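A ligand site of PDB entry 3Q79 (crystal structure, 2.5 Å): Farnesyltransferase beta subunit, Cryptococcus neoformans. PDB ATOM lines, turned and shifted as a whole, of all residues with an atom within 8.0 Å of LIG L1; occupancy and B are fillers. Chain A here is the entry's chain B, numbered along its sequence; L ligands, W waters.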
ATOM      1  N   LEU A  50     -17.898  10.682   6.273  1.00  0.00           N
ATOM      2  CA  LEU A  50     -19.003   9.919   6.828  1.00  0.00           C
ATOM      3  C   LEU A  50     -19.622  10.633   8.019  1.00  0.00           C
ATOM      4  O   LEU A  50     -20.600  11.362   7.885  1.00  0.00           O
ATOM      5  CB  LEU A  50     -18.533   8.520   7.242  1.00  0.00           C
ATOM      6  CG  LEU A  50     -18.216   7.549   6.107  1.00  0.00           C
ATOM      7  CD1 LEU A  50     -17.364   6.395   6.607  1.00  0.00           C
ATOM      8  CD2 LEU A  50     -19.504   7.036   5.478  1.00  0.00           C
ATOM      9  N   TYR A  58     -26.040  18.294   1.279  1.00  0.00           N
ATOM     10  CA  TYR A  58     -25.581  17.013   0.766  1.00  0.00           C
ATOM     11  C   TYR A  58     -25.295  17.098  -0.732  1.00  0.00           C
ATOM     12  O   TYR A  58     -26.152  17.511  -1.516  1.00  0.00           O
ATOM     13  CB  TYR A  58     -26.623  15.915   1.056  1.00  0.00           C
ATOM     14  CG  TYR A  58     -26.197  14.552   0.561  1.00  0.00           C
ATOM     15  CD1 TYR A  58     -26.954  13.861  -0.381  1.00  0.00           C
ATOM     16  CD2 TYR A  58     -25.037  13.945   1.030  1.00  0.00           C
ATOM     17  CE1 TYR A  58     -26.569  12.615  -0.845  1.00  0.00           C
ATOM     18  CE2 TYR A  58     -24.643  12.699   0.572  1.00  0.00           C
ATOM     19  CZ  TYR A  58     -25.407  12.037  -0.359  1.00  0.00           C
ATOM     20  OH  TYR A  58     -25.017  10.798  -0.811  1.00  0.00           O
ATOM     21  N   GLY A  60     -24.758  14.789  -2.948  1.00  0.00           N
ATOM     22  CA  GLY A  60     -25.156  13.657  -3.761  1.00  0.00           C
ATOM     23  C   GLY A  60     -25.767  14.063  -5.095  1.00  0.00           C
ATOM     24  O   GLY A  60     -26.451  15.080  -5.171  1.00  0.00           O
ATOM     25  N   LEU A  61     -25.517  13.277  -6.126  1.00  0.00           N
ATOM     26  CA  LEU A  61     -26.035  13.569  -7.461  1.00  0.00           C
ATOM     27  C   LEU A  61     -27.559  13.474  -7.476  1.00  0.00           C
ATOM     28  O   LEU A  61     -28.129  12.382  -7.388  1.00  0.00           O
ATOM     29  CB  LEU A  61     -25.437  12.624  -8.499  1.00  0.00           C
ATOM     30  CG  LEU A  61     -25.810  12.916  -9.956  1.00  0.00           C
ATOM     31  CD1 LEU A  61     -25.275  14.270 -10.384  1.00  0.00           C
ATOM     32  CD2 LEU A  61     -25.305  11.810 -10.874  1.00  0.00           C
ATOM     33  N   ILE A 486     -15.721   6.419  -7.876  1.00  0.00           N
ATOM     34  CA  ILE A 486     -17.020   7.067  -7.732  1.00  0.00           C
ATOM     35  C   ILE A 486     -17.128   7.865  -6.442  1.00  0.00           C
ATOM     36  O   ILE A 486     -17.552   7.353  -5.416  1.00  0.00           O
ATOM     37  CB  ILE A 486     -18.165   6.044  -7.776  1.00  0.00           C
ATOM     38  CG1 ILE A 486     -17.948   5.053  -8.915  1.00  0.00           C
ATOM     39  CG2 ILE A 486     -19.504   6.762  -7.918  1.00  0.00           C
ATOM     40  CD1 ILE A 486     -17.960   5.684 -10.282  1.00  0.00           C
ATOM     41  N   VAL A 487     -16.748   9.144  -6.511  1.00  0.00           N
ATOM     42  CA  VAL A 487     -16.788  10.007  -5.335  1.00  0.00           C
ATOM     43  C   VAL A 487     -18.196  10.108  -4.759  1.00  0.00           C
ATOM     44  O   VAL A 487     -19.164  10.304  -5.486  1.00  0.00           O
ATOM     45  CB  VAL A 487     -16.284  11.421  -5.667  1.00  0.00           C
ATOM     46  CG1 VAL A 487     -16.634  12.381  -4.539  1.00  0.00           C
ATOM     47  CG2 VAL A 487     -14.794  11.409  -5.930  1.00  0.00           C
ATOM     48  N   GLY A 488     -18.298   9.941  -3.443  1.00  0.00           N
ATOM     49  CA  GLY A 488     -19.555  10.129  -2.742  1.00  0.00           C
ATOM     50  C   GLY A 488     -20.444   8.902  -2.646  1.00  0.00           C
ATOM     51  O   GLY A 488     -21.531   8.968  -2.064  1.00  0.00           O
ATOM     52  N   GLY A 489     -19.998   7.784  -3.208  1.00  0.00           N
ATOM     53  CA  GLY A 489     -20.762   6.560  -3.160  1.00  0.00           C
ATOM     54  C   GLY A 489     -21.334   6.132  -4.498  1.00  0.00           C
ATOM     55  O   GLY A 489     -21.519   6.954  -5.407  1.00  0.00           O
ATOM     56  N   LYS A 490     -21.646   4.852  -4.617  1.00  0.00           N
ATOM     57  CA  LYS A 490     -22.066   4.263  -5.889  1.00  0.00           C
ATOM     58  C   LYS A 490     -23.377   4.831  -6.444  1.00  0.00           C
ATOM     59  O   LYS A 490     -23.646   4.699  -7.636  1.00  0.00           O
ATOM     60  CB  LYS A 490     -22.134   2.730  -5.759  1.00  0.00           C
ATOM     61  CG  LYS A 490     -20.771   2.089  -5.525  1.00  0.00           C
ATOM     62  CD  LYS A 490     -20.861   0.571  -5.447  1.00  0.00           C
ATOM     63  CE  LYS A 490     -19.478  -0.043  -5.236  1.00  0.00           C
ATOM     64  NZ  LYS A 490     -19.543  -1.534  -5.089  1.00  0.00           N
ATOM     65  N   ASP A 491     -24.164   5.457  -5.587  1.00  0.00           N
ATOM     66  CA  ASP A 491     -25.413   6.086  -6.018  1.00  0.00           C
ATOM     67  C   ASP A 491     -25.146   7.323  -6.882  1.00  0.00           C
ATOM     68  O   ASP A 491     -26.063   7.871  -7.491  1.00  0.00           O
ATOM     69  CB  ASP A 491     -26.288   6.460  -4.826  1.00  0.00           C
ATOM     70  CG  ASP A 491     -26.958   5.248  -4.208  1.00  0.00           C
ATOM     71  OD1 ASP A 491     -27.423   4.371  -4.958  1.00  0.00           O
ATOM     72  OD2 ASP A 491     -27.013   5.168  -2.961  1.00  0.00           O
ATOM     73  N   ASN A 492     -23.889   7.759  -6.912  1.00  0.00           N
ATOM     74  CA  ASN A 492     -23.485   8.871  -7.769  1.00  0.00           C
ATOM     75  C   ASN A 492     -23.063   8.392  -9.156  1.00  0.00           C
ATOM     76  O   ASN A 492     -23.007   9.185 -10.102  1.00  0.00           O
ATOM     77  CB  ASN A 492     -22.349   9.674  -7.126  1.00  0.00           C
ATOM     78  CG  ASN A 492     -22.818  10.552  -5.984  1.00  0.00           C
ATOM     79  OD1 ASN A 492     -23.982  10.952  -5.941  1.00  0.00           O
ATOM     80  ND2 ASN A 492     -21.918  10.840  -5.053  1.00  0.00           N
ATOM     81  N   ARG A 493     -22.751   7.114  -9.263  1.00  0.00           N
ATOM     82  CA  ARG A 493     -22.305   6.542 -10.526  1.00  0.00           C
ATOM     83  C   ARG A 493     -23.260   6.838 -11.687  1.00  0.00           C
ATOM     84  O   ARG A 493     -24.478   6.697 -11.563  1.00  0.00           O
ATOM     85  CB  ARG A 493     -22.138   5.024 -10.405  1.00  0.00           C
ATOM     86  CG  ARG A 493     -21.186   4.425 -11.441  1.00  0.00           C
ATOM     87  CD  ARG A 493     -21.465   2.949 -11.671  1.00  0.00           C
ATOM     88  NE  ARG A 493     -22.337   2.734 -12.827  1.00  0.00           N
ATOM     89  CZ  ARG A 493     -21.908   2.292 -14.006  1.00  0.00           C
ATOM     90  NH1 ARG A 493     -20.632   1.980 -14.185  1.00  0.00           N
ATOM     91  NH2 ARG A 493     -22.773   2.135 -15.001  1.00  0.00           N
HETATM   92  O1  LIG L   1     -21.209   1.697  -0.474  1.00  0.00           O
HETATM   93  O2  LIG L   1     -22.644   1.756  -2.464  1.00  0.00           O
HETATM   94  O3  LIG L   1     -24.291   4.385  -2.357  1.00  0.00           O
HETATM   95  O4  LIG L   1     -21.047   3.539  -2.027  1.00  0.00           O
HETATM   96  C1  LIG L   1     -29.237   8.033   0.749  1.00  0.00           C
HETATM   97  C2  LIG L   1     -28.708   6.751   1.280  1.00  0.00           C
HETATM   98  C3  LIG L   1     -28.347   8.903  -0.074  1.00  0.00           C
HETATM   99  C4  LIG L   1     -27.454   6.194   0.693  1.00  0.00           C
HETATM  100  C5  LIG L   1     -27.108   8.327  -0.643  1.00  0.00           C
HETATM  101  C6  LIG L   1     -24.833   5.464  -0.342  1.00  0.00           C
HETATM  102  C7  LIG L   1     -23.239   3.450  -0.466  1.00  0.00           C
HETATM  103  N1  LIG L   1     -25.754   6.374  -1.008  1.00  0.00           N
HETATM  104  C8  LIG L   1     -24.226   4.351  -1.146  1.00  0.00           C
HETATM  105  C9  LIG L   1     -26.506   7.133   0.015  1.00  0.00           C
HETATM  106  S1  LIG L   1     -21.989   2.592  -1.406  1.00  0.00           S
HETATM  107  O1  LG2 L   2     -33.240  13.933  -7.486  1.00  0.00           O
HETATM  108  O2  LG2 L   2     -32.635  14.631  -5.226  1.00  0.00           O
HETATM  109  O3  LG2 L   2     -35.259  15.115  -4.673  1.00  0.00           O
HETATM  110  O4  LG2 L   2     -32.200  12.363  -5.973  1.00  0.00           O
HETATM  111  C1  LG2 L   2     -39.942  12.001   0.019  1.00  0.00           C
HETATM  112  C2  LG2 L   2     -39.827  13.449  -0.328  1.00  0.00           C
HETATM  113  C3  LG2 L   2     -39.237  10.999  -0.817  1.00  0.00           C
HETATM  114  C4  LG2 L   2     -39.150  13.836  -1.597  1.00  0.00           C
HETATM  115  C5  LG2 L   2     -38.176  11.478  -1.739  1.00  0.00           C
HETATM  116  C6  LG2 L   2     -36.924  13.548  -4.145  1.00  0.00           C
HETATM  117  C7  LG2 L   2     -34.744  12.959  -5.447  1.00  0.00           C
HETATM  118  N1  LG2 L   2     -37.005  13.359  -2.694  1.00  0.00           N
HETATM  119  C8  LG2 L   2     -35.613  13.973  -4.755  1.00  0.00           C
HETATM  120  C9  LG2 L   2     -38.356  12.821  -2.355  1.00  0.00           C
HETATM  121  S1  LG2 L   2     -33.150  13.481  -6.054  1.00  0.00           S
HETATM  122  O   HOH W   1     -23.840   7.664  -2.644  1.00  0.00           O
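The backbone NH (N) of Asp 491 lies close to an oxygen (O3) of LIG L1, at 3.4 Å.
The side-chain carboxylate (OD2) of Asp 491 lies within salt-bridge range of a nitrogen (N1) of LIG L1 (2.6 Å).
The backbone NH (N) of Lys 490 is in hydrogen-bond range of an oxygen (O4) of LIG L1.
Tyr 58 touches LIG L1 (OH to C5, 3.2 Å).
Gly 489 touches LIG L1 (CA to O4, 3.2 Å).
The nearest printed residue that does not touch LIG L1 is Gly 488 (5.1 Å).
Water W1 bridges O of Gly 488 and N1 of LIG L1.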
